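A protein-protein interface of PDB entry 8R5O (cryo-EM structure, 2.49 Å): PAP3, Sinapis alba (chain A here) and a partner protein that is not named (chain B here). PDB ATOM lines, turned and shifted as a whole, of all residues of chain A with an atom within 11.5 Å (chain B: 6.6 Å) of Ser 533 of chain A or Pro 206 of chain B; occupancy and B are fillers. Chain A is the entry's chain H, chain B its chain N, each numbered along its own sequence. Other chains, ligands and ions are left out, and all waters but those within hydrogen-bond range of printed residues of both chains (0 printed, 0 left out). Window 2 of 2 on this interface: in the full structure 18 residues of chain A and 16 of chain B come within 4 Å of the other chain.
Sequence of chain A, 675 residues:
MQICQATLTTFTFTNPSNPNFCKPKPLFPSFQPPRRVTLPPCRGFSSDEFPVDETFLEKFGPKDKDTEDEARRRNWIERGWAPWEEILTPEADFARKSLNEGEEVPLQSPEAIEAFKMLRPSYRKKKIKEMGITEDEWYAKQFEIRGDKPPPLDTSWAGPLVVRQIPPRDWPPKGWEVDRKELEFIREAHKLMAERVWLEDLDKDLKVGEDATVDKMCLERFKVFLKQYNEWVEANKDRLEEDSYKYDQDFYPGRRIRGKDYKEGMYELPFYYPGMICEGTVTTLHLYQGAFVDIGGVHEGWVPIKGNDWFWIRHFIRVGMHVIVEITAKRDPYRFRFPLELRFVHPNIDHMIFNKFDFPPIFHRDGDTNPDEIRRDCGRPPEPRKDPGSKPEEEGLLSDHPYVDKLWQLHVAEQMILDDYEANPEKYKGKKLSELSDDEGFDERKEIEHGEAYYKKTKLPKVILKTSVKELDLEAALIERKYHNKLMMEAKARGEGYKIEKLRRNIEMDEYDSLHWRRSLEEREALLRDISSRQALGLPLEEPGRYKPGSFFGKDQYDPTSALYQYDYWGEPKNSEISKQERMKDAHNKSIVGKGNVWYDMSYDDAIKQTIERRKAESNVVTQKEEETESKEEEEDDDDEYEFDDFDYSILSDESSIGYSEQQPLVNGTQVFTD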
ATOM      1  N   ARG A 524      23.746  -4.601 -31.673  1.00  0.00           N
ATOM      2  CA  ARG A 524      22.329  -4.366 -31.934  1.00  0.00           C
ATOM      3  C   ARG A 524      21.699  -5.535 -32.677  1.00  0.00           C
ATOM      4  O   ARG A 524      20.568  -5.933 -32.379  1.00  0.00           O
ATOM      5  CB  ARG A 524      22.149  -3.070 -32.723  1.00  0.00           C
ATOM      6  CG  ARG A 524      20.698  -2.703 -32.987  1.00  0.00           C
ATOM      7  CD  ARG A 524      19.926  -2.537 -31.692  1.00  0.00           C
ATOM      8  NE  ARG A 524      20.568  -1.579 -30.800  1.00  0.00           N
ATOM      9  CZ  ARG A 524      20.371  -0.269 -30.841  1.00  0.00           C
ATOM     10  NH1 ARG A 524      19.542   0.279 -31.714  1.00  0.00           N
ATOM     11  NH2 ARG A 524      21.025   0.512 -29.986  1.00  0.00           N
ATOM     12  N   GLU A 525      22.414  -6.095 -33.657  1.00  0.00           N
ATOM     13  CA  GLU A 525      21.891  -7.244 -34.388  1.00  0.00           C
ATOM     14  C   GLU A 525      21.702  -8.444 -33.469  1.00  0.00           C
ATOM     15  O   GLU A 525      20.688  -9.146 -33.554  1.00  0.00           O
ATOM     16  CB  GLU A 525      22.821  -7.593 -35.549  1.00  0.00           C
ATOM     17  CG  GLU A 525      22.817  -6.570 -36.667  1.00  0.00           C
ATOM     18  CD  GLU A 525      23.839  -6.877 -37.741  1.00  0.00           C
ATOM     19  OE1 GLU A 525      24.934  -7.373 -37.400  1.00  0.00           O
ATOM     20  OE2 GLU A 525      23.547  -6.627 -38.930  1.00  0.00           O
ATOM     21  N   ALA A 526      22.668  -8.696 -32.585  1.00  0.00           N
ATOM     22  CA  ALA A 526      22.510  -9.764 -31.606  1.00  0.00           C
ATOM     23  C   ALA A 526      21.404  -9.446 -30.609  1.00  0.00           C
ATOM     24  O   ALA A 526      20.711 -10.358 -30.146  1.00  0.00           O
ATOM     25  CB  ALA A 526      23.829 -10.013 -30.877  1.00  0.00           C
ATOM     26  N   LEU A 527      21.225  -8.168 -30.270  1.00  0.00           N
ATOM     27  CA  LEU A 527      20.156  -7.786 -29.353  1.00  0.00           C
ATOM     28  C   LEU A 527      18.784  -8.062 -29.953  1.00  0.00           C
ATOM     29  O   LEU A 527      17.871  -8.510 -29.251  1.00  0.00           O
ATOM     30  CB  LEU A 527      20.290  -6.311 -28.977  1.00  0.00           C
ATOM     31  CG  LEU A 527      19.198  -5.734 -28.072  1.00  0.00           C
ATOM     32  CD1 LEU A 527      19.141  -6.484 -26.751  1.00  0.00           C
ATOM     33  CD2 LEU A 527      19.418  -4.250 -27.843  1.00  0.00           C
ATOM     34  N   LEU A 528      18.619  -7.796 -31.251  1.00  0.00           N
ATOM     35  CA  LEU A 528      17.327  -8.018 -31.893  1.00  0.00           C
ATOM     36  C   LEU A 528      16.948  -9.493 -31.889  1.00  0.00           C
ATOM     37  O   LEU A 528      15.787  -9.838 -31.641  1.00  0.00           O
ATOM     38  CB  LEU A 528      17.353  -7.470 -33.320  1.00  0.00           C
ATOM     39  CG  LEU A 528      17.498  -5.951 -33.438  1.00  0.00           C
ATOM     40  CD1 LEU A 528      17.743  -5.547 -34.881  1.00  0.00           C
ATOM     41  CD2 LEU A 528      16.270  -5.247 -32.885  1.00  0.00           C
ATOM     42  N   ARG A 529      17.907 -10.378 -32.166  1.00  0.00           N
ATOM     43  CA  ARG A 529      17.636 -11.809 -32.062  1.00  0.00           C
ATOM     44  C   ARG A 529      17.405 -12.220 -30.614  1.00  0.00           C
ATOM     45  O   ARG A 529      16.546 -13.061 -30.330  1.00  0.00           O
ATOM     46  CB  ARG A 529      18.781 -12.615 -32.670  1.00  0.00           C
ATOM     47  CG  ARG A 529      19.141 -12.220 -34.089  1.00  0.00           C
ATOM     48  CD  ARG A 529      19.950 -13.306 -34.772  1.00  0.00           C
ATOM     49  NE  ARG A 529      20.894 -13.940 -33.861  1.00  0.00           N
ATOM     50  CZ  ARG A 529      22.114 -13.487 -33.609  1.00  0.00           C
ATOM     51  NH1 ARG A 529      22.575 -12.388 -34.182  1.00  0.00           N
ATOM     52  NH2 ARG A 529      22.889 -14.152 -32.759  1.00  0.00           N
ATOM     53  N   ASP A 530      18.165 -11.635 -29.684  1.00  0.00           N
ATOM     54  CA  ASP A 530      18.003 -11.971 -28.273  1.00  0.00           C
ATOM     55  C   ASP A 530      16.623 -11.574 -27.766  1.00  0.00           C
ATOM     56  O   ASP A 530      16.040 -12.268 -26.926  1.00  0.00           O
ATOM     57  CB  ASP A 530      19.097 -11.295 -27.446  1.00  0.00           C
ATOM     58  CG  ASP A 530      19.120 -11.774 -26.010  1.00  0.00           C
ATOM     59  OD1 ASP A 530      19.503 -12.938 -25.777  1.00  0.00           O
ATOM     60  OD2 ASP A 530      18.757 -10.986 -25.112  1.00  0.00           O
ATOM     61  N   ILE A 531      16.086 -10.458 -28.261  1.00  0.00           N
ATOM     62  CA  ILE A 531      14.754 -10.023 -27.849  1.00  0.00           C
ATOM     63  C   ILE A 531      13.701 -11.032 -28.295  1.00  0.00           C
ATOM     64  O   ILE A 531      12.811 -11.406 -27.524  1.00  0.00           O
ATOM     65  CB  ILE A 531      14.458  -8.613 -28.393  1.00  0.00           C
ATOM     66  CG1 ILE A 531      15.275  -7.570 -27.633  1.00  0.00           C
ATOM     67  CG2 ILE A 531      12.975  -8.296 -28.304  1.00  0.00           C
ATOM     68  CD1 ILE A 531      15.105  -6.167 -28.156  1.00  0.00           C
ATOM     69  N   SER A 532      13.795 -11.496 -29.543  1.00  0.00           N
ATOM     70  CA  SER A 532      12.796 -12.426 -30.062  1.00  0.00           C
ATOM     71  C   SER A 532      12.813 -13.747 -29.301  1.00  0.00           C
ATOM     72  O   SER A 532      11.754 -14.321 -29.026  1.00  0.00           O
ATOM     73  CB  SER A 532      13.018 -12.661 -31.557  1.00  0.00           C
ATOM     74  OG  SER A 532      14.278 -13.250 -31.813  1.00  0.00           O
ATOM     75  N   SER A 533      14.002 -14.247 -28.958  1.00  0.00           N
ATOM     76  CA  SER A 533      14.092 -15.489 -28.195  1.00  0.00           C
ATOM     77  C   SER A 533      13.510 -15.325 -26.797  1.00  0.00           C
ATOM     78  O   SER A 533      12.768 -16.188 -26.317  1.00  0.00           O
ATOM     79  CB  SER A 533      15.546 -15.956 -28.119  1.00  0.00           C
ATOM     80  OG  SER A 533      16.069 -16.215 -29.408  1.00  0.00           O
ATOM     81  N   ARG A 534      13.840 -14.219 -26.124  1.00  0.00           N
ATOM     82  CA  ARG A 534      13.374 -14.020 -24.754  1.00  0.00           C
ATOM     83  C   ARG A 534      11.872 -13.771 -24.702  1.00  0.00           C
ATOM     84  O   ARG A 534      11.197 -14.226 -23.774  1.00  0.00           O
ATOM     85  CB  ARG A 534      14.137 -12.867 -24.106  1.00  0.00           C
ATOM     86  CG  ARG A 534      15.589 -13.195 -23.821  1.00  0.00           C
ATOM     87  CD  ARG A 534      16.314 -12.037 -23.169  1.00  0.00           C
ATOM     88  NE  ARG A 534      17.659 -12.421 -22.763  1.00  0.00           N
ATOM     89  CZ  ARG A 534      17.968 -12.925 -21.576  1.00  0.00           C
ATOM     90  NH1 ARG A 534      17.051 -13.093 -20.638  1.00  0.00           N
ATOM     91  NH2 ARG A 534      19.227 -13.267 -21.324  1.00  0.00           N
ATOM     92  N   GLN A 535      11.332 -13.042 -25.682  1.00  0.00           N
ATOM     93  CA  GLN A 535       9.891 -12.813 -25.712  1.00  0.00           C
ATOM     94  C   GLN A 535       9.123 -14.100 -25.983  1.00  0.00           C
ATOM     95  O   GLN A 535       8.002 -14.266 -25.491  1.00  0.00           O
ATOM     96  CB  GLN A 535       9.544 -11.758 -26.762  1.00  0.00           C
ATOM     97  CG  GLN A 535      10.046 -10.356 -26.445  1.00  0.00           C
ATOM     98  CD  GLN A 535       9.152  -9.602 -25.478  1.00  0.00           C
ATOM     99  OE1 GLN A 535       8.667 -10.158 -24.494  1.00  0.00           O
ATOM    100  NE2 GLN A 535       8.927  -8.325 -25.759  1.00  0.00           N
ATOM    101  N   ALA A 536       9.704 -15.016 -26.758  1.00  0.00           N
ATOM    102  CA  ALA A 536       9.042 -16.283 -27.044  1.00  0.00           C
ATOM    103  C   ALA A 536       9.088 -17.228 -25.850  1.00  0.00           C
ATOM    104  O   ALA A 536       8.144 -17.993 -25.624  1.00  0.00           O
ATOM    105  CB  ALA A 536       9.674 -16.942 -28.268  1.00  0.00           C
ATOM    106  N   LEU A 537      10.171 -17.193 -25.080  1.00  0.00           N
ATOM    107  CA  LEU A 537      10.372 -18.110 -23.967  1.00  0.00           C
ATOM    108  C   LEU A 537      10.023 -17.500 -22.617  1.00  0.00           C
ATOM    109  O   LEU A 537      10.240 -18.146 -21.587  1.00  0.00           O
ATOM    110  CB  LEU A 537      11.821 -18.606 -23.956  1.00  0.00           C
ATOM    111  CG  LEU A 537      12.260 -19.324 -25.233  1.00  0.00           C
ATOM    112  CD1 LEU A 537      13.751 -19.596 -25.212  1.00  0.00           C
ATOM    113  CD2 LEU A 537      11.480 -20.617 -25.412  1.00  0.00           C
ATOM    114  N   GLY A 538       9.492 -16.282 -22.593  1.00  0.00           N
ATOM    115  CA  GLY A 538       9.119 -15.652 -21.337  1.00  0.00           C
ATOM    116  C   GLY A 538      10.285 -15.345 -20.425  1.00  0.00           C
ATOM    117  O   GLY A 538      10.173 -15.500 -19.203  1.00  0.00           O
ATOM    118  N   LEU A 539      11.406 -14.912 -20.990  1.00  0.00           N
ATOM    119  CA  LEU A 539      12.577 -14.512 -20.231  1.00  0.00           C
ATOM    120  C   LEU A 539      12.654 -12.993 -20.132  1.00  0.00           C
ATOM    121  O   LEU A 539      12.237 -12.284 -21.054  1.00  0.00           O
ATOM    122  CB  LEU A 539      13.853 -15.050 -20.884  1.00  0.00           C
ATOM    123  CG  LEU A 539      14.063 -16.562 -20.790  1.00  0.00           C
ATOM    124  CD1 LEU A 539      15.157 -17.010 -21.740  1.00  0.00           C
ATOM    125  CD2 LEU A 539      14.403 -16.963 -19.365  1.00  0.00           C
ATOM    126  N   PRO A 540      13.167 -12.461 -19.025  1.00  0.00           N
ATOM    127  CA  PRO A 540      13.180 -11.004 -18.847  1.00  0.00           C
ATOM    128  C   PRO A 540      14.057 -10.310 -19.879  1.00  0.00           C
ATOM    129  O   PRO A 540      15.111 -10.814 -20.271  1.00  0.00           O
ATOM    130  CB  PRO A 540      13.733 -10.827 -17.429  1.00  0.00           C
ATOM    131  CG  PRO A 540      14.523 -12.063 -17.179  1.00  0.00           C
ATOM    132  CD  PRO A 540      13.787 -13.160 -17.885  1.00  0.00           C
ATOM    133  N   LEU A 541      13.604  -9.137 -20.321  1.00  0.00           N
ATOM    134  CA  LEU A 541      14.393  -8.297 -21.213  1.00  0.00           C
ATOM    135  C   LEU A 541      15.335  -7.374 -20.456  1.00  0.00           C
ATOM    136  O   LEU A 541      16.440  -7.097 -20.935  1.00  0.00           O
ATOM    137  CB  LEU A 541      13.472  -7.467 -22.110  1.00  0.00           C
ATOM    138  CG  LEU A 541      12.602  -8.258 -23.088  1.00  0.00           C
ATOM    139  CD1 LEU A 541      11.762  -7.317 -23.935  1.00  0.00           C
ATOM    140  CD2 LEU A 541      13.465  -9.151 -23.963  1.00  0.00           C
ATOM    141  N   GLU A 542      14.919  -6.893 -19.291  1.00  0.00           N
ATOM    142  CA  GLU A 542      15.748  -6.081 -18.414  1.00  0.00           C
ATOM    143  C   GLU A 542      16.180  -6.913 -17.216  1.00  0.00           C
ATOM    144  O   GLU A 542      15.590  -7.951 -16.911  1.00  0.00           O
ATOM    145  CB  GLU A 542      14.995  -4.833 -17.941  1.00  0.00           C
ATOM    146  CG  GLU A 542      14.211  -4.120 -19.029  1.00  0.00           C
ATOM    147  CD  GLU A 542      15.101  -3.442 -20.052  1.00  0.00           C
ATOM    148  OE1 GLU A 542      16.285  -3.189 -19.744  1.00  0.00           O
ATOM    149  OE2 GLU A 542      14.614  -3.162 -21.168  1.00  0.00           O
ATOM    150  N   TYR B 106       4.195  -9.847 -35.468  1.00  0.00           N
ATOM    151  CA  TYR B 106       5.355  -9.848 -34.582  1.00  0.00           C
ATOM    152  C   TYR B 106       5.388  -8.588 -33.726  1.00  0.00           C
ATOM    153  O   TYR B 106       5.725  -8.649 -32.538  1.00  0.00           O
ATOM    154  CB  TYR B 106       6.643  -9.991 -35.391  1.00  0.00           C
ATOM    155  CG  TYR B 106       7.901  -9.952 -34.552  1.00  0.00           C
ATOM    156  CD1 TYR B 106       8.183 -10.959 -33.637  1.00  0.00           C
ATOM    157  CD2 TYR B 106       8.810  -8.912 -34.680  1.00  0.00           C
ATOM    158  CE1 TYR B 106       9.332 -10.925 -32.870  1.00  0.00           C
ATOM    159  CE2 TYR B 106       9.960  -8.871 -33.920  1.00  0.00           C
ATOM    160  CZ  TYR B 106      10.216  -9.877 -33.017  1.00  0.00           C
ATOM    161  OH  TYR B 106      11.363  -9.831 -32.261  1.00  0.00           O
ATOM    162  N   MET B 111       4.575  -9.720 -29.496  1.00  0.00           N
ATOM    163  CA  MET B 111       3.860 -10.524 -30.477  1.00  0.00           C
ATOM    164  C   MET B 111       2.356 -10.491 -30.242  1.00  0.00           C
ATOM    165  O   MET B 111       1.879 -10.639 -29.114  1.00  0.00           O
ATOM    166  CB  MET B 111       4.365 -11.967 -30.437  1.00  0.00           C
ATOM    167  CG  MET B 111       5.877 -12.096 -30.542  1.00  0.00           C
ATOM    168  SD  MET B 111       6.464 -13.788 -30.332  1.00  0.00           S
ATOM    169  CE  MET B 111       8.237 -13.535 -30.317  1.00  0.00           C
ATOM    170  N   ASN B 168      19.781 -26.922 -30.339  1.00  0.00           N
ATOM    171  CA  ASN B 168      18.599 -26.079 -30.199  1.00  0.00           C
ATOM    172  C   ASN B 168      17.679 -26.686 -29.144  1.00  0.00           C
ATOM    173  O   ASN B 168      17.008 -27.690 -29.400  1.00  0.00           O
ATOM    174  CB  ASN B 168      17.892 -25.942 -31.543  1.00  0.00           C
ATOM    175  CG  ASN B 168      16.969 -24.741 -31.601  1.00  0.00           C
ATOM    176  OD1 ASN B 168      16.983 -23.888 -30.715  1.00  0.00           O
ATOM    177  ND2 ASN B 168      16.168 -24.663 -32.656  1.00  0.00           N
ATOM    178  N   PHE B 169      17.646 -26.075 -27.964  1.00  0.00           N
ATOM    179  CA  PHE B 169      16.948 -26.651 -26.820  1.00  0.00           C
ATOM    180  C   PHE B 169      15.455 -26.364 -26.907  1.00  0.00           C
ATOM    181  O   PHE B 169      15.043 -25.217 -27.108  1.00  0.00           O
ATOM    182  CB  PHE B 169      17.525 -26.094 -25.517  1.00  0.00           C
ATOM    183  CG  PHE B 169      16.963 -26.732 -24.278  1.00  0.00           C
ATOM    184  CD1 PHE B 169      17.375 -27.993 -23.885  1.00  0.00           C
ATOM    185  CD2 PHE B 169      16.036 -26.062 -23.497  1.00  0.00           C
ATOM    186  CE1 PHE B 169      16.865 -28.578 -22.746  1.00  0.00           C
ATOM    187  CE2 PHE B 169      15.524 -26.642 -22.355  1.00  0.00           C
ATOM    188  CZ  PHE B 169      15.940 -27.902 -21.978  1.00  0.00           C
ATOM    189  N   SER B 171      11.548 -26.643 -28.491  1.00  0.00           N
ATOM    190  CA  SER B 171      10.993 -26.525 -29.830  1.00  0.00           C
ATOM    191  C   SER B 171      11.594 -25.322 -30.544  1.00  0.00           C
ATOM    192  O   SER B 171      11.759 -24.251 -29.954  1.00  0.00           O
ATOM    193  CB  SER B 171       9.472 -26.385 -29.765  1.00  0.00           C
ATOM    194  OG  SER B 171       8.884 -27.474 -29.079  1.00  0.00           O
ATOM    195  N   GLY B 172      11.922 -25.500 -31.817  1.00  0.00           N
ATOM    196  CA  GLY B 172      12.484 -24.401 -32.576  1.00  0.00           C
ATOM    197  C   GLY B 172      12.876 -24.827 -33.972  1.00  0.00           C
ATOM    198  O   GLY B 172      12.573 -25.935 -34.416  1.00  0.00           O
ATOM    199  N   TRP B 173      13.560 -23.915 -34.660  1.00  0.00           N
ATOM    200  CA  TRP B 173      14.000 -24.110 -36.033  1.00  0.00           C
ATOM    201  C   TRP B 173      15.452 -23.671 -36.167  1.00  0.00           C
ATOM    202  O   TRP B 173      15.907 -22.764 -35.468  1.00  0.00           O
ATOM    203  CB  TRP B 173      13.130 -23.317 -37.026  1.00  0.00           C
ATOM    204  CG  TRP B 173      11.665 -23.616 -36.947  1.00  0.00           C
ATOM    205  CD1 TRP B 173      10.797 -23.218 -35.975  1.00  0.00           C
ATOM    206  CD2 TRP B 173      10.892 -24.365 -37.891  1.00  0.00           C
ATOM    207  NE1 TRP B 173       9.534 -23.681 -36.247  1.00  0.00           N
ATOM    208  CE2 TRP B 173       9.565 -24.387 -37.420  1.00  0.00           C
ATOM    209  CE3 TRP B 173      11.192 -25.022 -39.087  1.00  0.00           C
ATOM    210  CZ2 TRP B 173       8.543 -25.044 -38.100  1.00  0.00           C
ATOM    211  CZ3 TRP B 173      10.176 -25.668 -39.761  1.00  0.00           C
ATOM    212  CH2 TRP B 173       8.868 -25.674 -39.267  1.00  0.00           C
ATOM    213  N   LYS B 204      19.577 -20.029 -34.941  1.00  0.00           N
ATOM    214  CA  LYS B 204      18.563 -20.845 -34.291  1.00  0.00           C
ATOM    215  C   LYS B 204      17.468 -19.946 -33.736  1.00  0.00           C
ATOM    216  O   LYS B 204      17.747 -18.859 -33.224  1.00  0.00           O
ATOM    217  CB  LYS B 204      19.167 -21.681 -33.161  1.00  0.00           C
ATOM    218  CG  LYS B 204      20.404 -22.455 -33.555  1.00  0.00           C
ATOM    219  CD  LYS B 204      20.897 -23.310 -32.403  1.00  0.00           C
ATOM    220  CE  LYS B 204      21.200 -22.479 -31.175  1.00  0.00           C
ATOM    221  NZ  LYS B 204      21.631 -23.325 -30.034  1.00  0.00           N
ATOM    222  N   THR B 205      16.226 -20.398 -33.844  1.00  0.00           N
ATOM    223  CA  THR B 205      15.098 -19.667 -33.296  1.00  0.00           C
ATOM    224  C   THR B 205      14.261 -20.594 -32.428  1.00  0.00           C
ATOM    225  O   THR B 205      14.202 -21.801 -32.681  1.00  0.00           O
ATOM    226  CB  THR B 205      14.213 -19.074 -34.402  1.00  0.00           C
ATOM    227  OG1 THR B 205      13.619 -20.132 -35.163  1.00  0.00           O
ATOM    228  CG2 THR B 205      15.024 -18.190 -35.327  1.00  0.00           C
ATOM    229  N   PRO B 206      13.619 -20.063 -31.393  1.00  0.00           N
ATOM    230  CA  PRO B 206      12.719 -20.875 -30.572  1.00  0.00           C
ATOM    231  C   PRO B 206      11.275 -20.814 -31.044  1.00  0.00           C
ATOM    232  O   PRO B 206      10.794 -19.799 -31.552  1.00  0.00           O
ATOM    233  CB  PRO B 206      12.864 -20.237 -29.185  1.00  0.00           C
ATOM    234  CG  PRO B 206      13.111 -18.804 -29.482  1.00  0.00           C
ATOM    235  CD  PRO B 206      13.902 -18.758 -30.769  1.00  0.00           C
ATOM    236  N   ASN B 207      10.586 -21.941 -30.864  1.00  0.00           N
ATOM    237  CA  ASN B 207       9.155 -22.063 -31.126  1.00  0.00           C
ATOM    238  C   ASN B 207       8.783 -21.691 -32.559  1.00  0.00           C
ATOM    239  O   ASN B 207       9.071 -22.442 -33.493  1.00  0.00           O
ATOM    240  CB  ASN B 207       8.362 -21.210 -30.133  1.00  0.00           C
ATOM    241  CG  ASN B 207       8.503 -21.699 -28.705  1.00  0.00           C
ATOM    242  OD1 ASN B 207       8.838 -22.858 -28.464  1.00  0.00           O
ATOM    243  ND2 ASN B 207       8.243 -20.819 -27.748  1.00  0.00           N
ATOM    244  N   ALA B 208       8.133 -20.542 -32.739  1.00  0.00           N
ATOM    245  CA  ALA B 208       7.617 -20.131 -34.036  1.00  0.00           C
ATOM    246  C   ALA B 208       8.429 -19.026 -34.696  1.00  0.00           C
ATOM    247  O   ALA B 208       8.102 -18.627 -35.817  1.00  0.00           O
ATOM    248  CB  ALA B 208       6.157 -19.682 -33.905  1.00  0.00           C
ATOM    249  N   VAL B 209       9.474 -18.522 -34.041  1.00  0.00           N
ATOM    250  CA  VAL B 209      10.234 -17.404 -34.582  1.00  0.00           C
ATOM    251  C   VAL B 209      10.978 -17.839 -35.839  1.00  0.00           C
ATOM    252  O   VAL B 209      11.462 -18.973 -35.937  1.00  0.00           O
ATOM    253  CB  VAL B 209      11.195 -16.856 -33.514  1.00  0.00           C
ATOM    254  CG1 VAL B 209      11.984 -15.670 -34.045  1.00  0.00           C
ATOM    255  CG2 VAL B 209      10.423 -16.468 -32.262  1.00  0.00           C
ATOM    256  N   ASN B 210      11.053 -16.943 -36.815  1.00  0.00           N
ATOM    257  CA  ASN B 210      11.777 -17.160 -38.055  1.00  0.00           C
ATOM    258  C   ASN B 210      12.605 -15.919 -38.355  1.00  0.00           C
ATOM    259  O   ASN B 210      12.338 -14.844 -37.807  1.00  0.00           O
ATOM    260  CB  ASN B 210      10.825 -17.479 -39.220  1.00  0.00           C
ATOM    261  CG  ASN B 210       9.690 -16.481 -39.351  1.00  0.00           C
ATOM    262  OD1 ASN B 210       9.883 -15.275 -39.222  1.00  0.00           O
ATOM    263  ND2 ASN B 210       8.492 -16.990 -39.614  1.00  0.00           N
ATOM    264  N   TRP B 214      13.712 -10.283 -38.370  1.00  0.00           N
ATOM    265  CA  TRP B 214      14.895  -9.434 -38.356  1.00  0.00           C
ATOM    266  C   TRP B 214      15.305  -8.988 -39.752  1.00  0.00           C
ATOM    267  O   TRP B 214      16.428  -8.506 -39.931  1.00  0.00           O
ATOM    268  CB  TRP B 214      16.079 -10.135 -37.688  1.00  0.00           C
ATOM    269  CG  TRP B 214      15.726 -11.117 -36.626  1.00  0.00           C
ATOM    270  CD1 TRP B 214      14.971 -10.894 -35.515  1.00  0.00           C
ATOM    271  CD2 TRP B 214      16.148 -12.481 -36.560  1.00  0.00           C
ATOM    272  NE1 TRP B 214      14.882 -12.042 -34.768  1.00  0.00           N
ATOM    273  CE2 TRP B 214      15.598 -13.032 -35.388  1.00  0.00           C
ATOM    274  CE3 TRP B 214      16.935 -13.292 -37.382  1.00  0.00           C
ATOM    275  CZ2 TRP B 214      15.808 -14.354 -35.019  1.00  0.00           C
ATOM    276  CZ3 TRP B 214      17.141 -14.604 -37.014  1.00  0.00           C
ATOM    277  CH2 TRP B 214      16.581 -15.123 -35.843  1.00  0.00           C
ATOM    278  N   TRP B 225      11.061 -29.165 -33.819  1.00  0.00           N
ATOM    279  CA  TRP B 225       9.973 -29.566 -32.942  1.00  0.00           C
ATOM    280  C   TRP B 225       9.926 -31.086 -32.881  1.00  0.00           C
ATOM    281  O   TRP B 225      10.163 -31.768 -33.881  1.00  0.00           O
ATOM    282  CB  TRP B 225       8.636 -29.017 -33.444  1.00  0.00           C
ATOM    283  CG  TRP B 225       8.430 -27.543 -33.225  1.00  0.00           C
ATOM    284  CD1 TRP B 225       9.190 -26.526 -33.720  1.00  0.00           C
ATOM    285  CD2 TRP B 225       7.371 -26.928 -32.484  1.00  0.00           C
ATOM    286  NE1 TRP B 225       8.682 -25.317 -33.321  1.00  0.00           N
ATOM    287  CE2 TRP B 225       7.564 -25.534 -32.561  1.00  0.00           C
ATOM    288  CE3 TRP B 225       6.285 -27.418 -31.755  1.00  0.00           C
ATOM    289  CZ2 TRP B 225       6.710 -24.629 -31.937  1.00  0.00           C
ATOM    290  CZ3 TRP B 225       5.441 -26.519 -31.137  1.00  0.00           C
ATOM    291  CH2 TRP B 225       5.656 -25.139 -31.231  1.00  0.00           C
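The backbone carbonyl oxygen of Tyr 106 of chain B sits close to the backbone NH of Met 111 of chain B (3.4 Å). The backbone carbonyl oxygen of Arg 529 of chain A lies within hydrogen-bond range of the side-chain hydroxyl of Ser 532 of chain A, 2.7 Å away. The indole nitrogen (NE1) of Trp 173 of chain B sits at hydrogen-bond distance from the backbone carbonyl oxygen (O) of Asn 207 of chain B (3.1 Å). O of Asn 207 of chain B lies within hydrogen-bond range of NE1 of Trp 225 of chain B (2.9 Å). The backbone carbonyl oxygen of Arg 529 of chain A lies within hydrogen-bond range of the side-chain hydroxyl of Ser 533 of chain A. O of Ser 171 of chain B lies within hydrogen-bond range of N of Asn 207 of chain B (2.7 Å).
Of the 19 printed residues of chain A, 6 touch a printed residue of chain B. Printed residues of chain A that touch a printed residue of chain B: Leu 528, Arg 529, Ser 532, Ser 533, Ala 536 and Leu 537. Hydrophobic or aromatic side chains of chain B within 4 Å of the printed part of chain A: Tyr 106, Met 111, Pro 206 and Trp 214.
The indole nitrogen (NE1) of Trp 214 of chain B sits at hydrogen-bond distance from the side-chain hydroxyl (OG) of Ser 532 of chain A, at 3.2 Å.
Among the printed residues, pairs that only touch across the chains: Ser 532 of chain A with Tyr 106 of chain B (3.4 Å), Ala 536 of chain A with Asn 207 of chain B (3.5 Å), Ser 533 of chain A with Pro 206 of chain B (3.6 Å), Arg 529 of chain A with Trp 214 of chain B (3.8 Å), Ser 532 of chain A with Met 111 of chain B (3.8 Å), Leu 528 of chain A with Trp 214 of chain B (3.9 Å) and Leu 537 of chain A with Asn 207 of chain B (3.997 Å).
Printed residues of chain B within 4 Å of Leu 528 of chain A: Trp 214. Of chain B, only Pro 206 (3.6 Å) comes within 4 Å of Ser 533 of chain A. Gly 538 of chain A touches none of the printed residues of chain B. Printed residues of chain A within 4 Å of Met 111 of chain B: Ser 532. No residue of chain A comes within 4 Å of Gly 172 of chain B. No residue of chain A comes within 4 Å of Thr 205 of chain B. No residue of chain A comes within 4 Å of Ala 208 of chain B. Asn 210 of chain B touches none of the printed residues of chain A. The nearest printed residue of chain A that does not touch Asn 207 of chain B is Ser 533 of chain A (6.6 Å).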
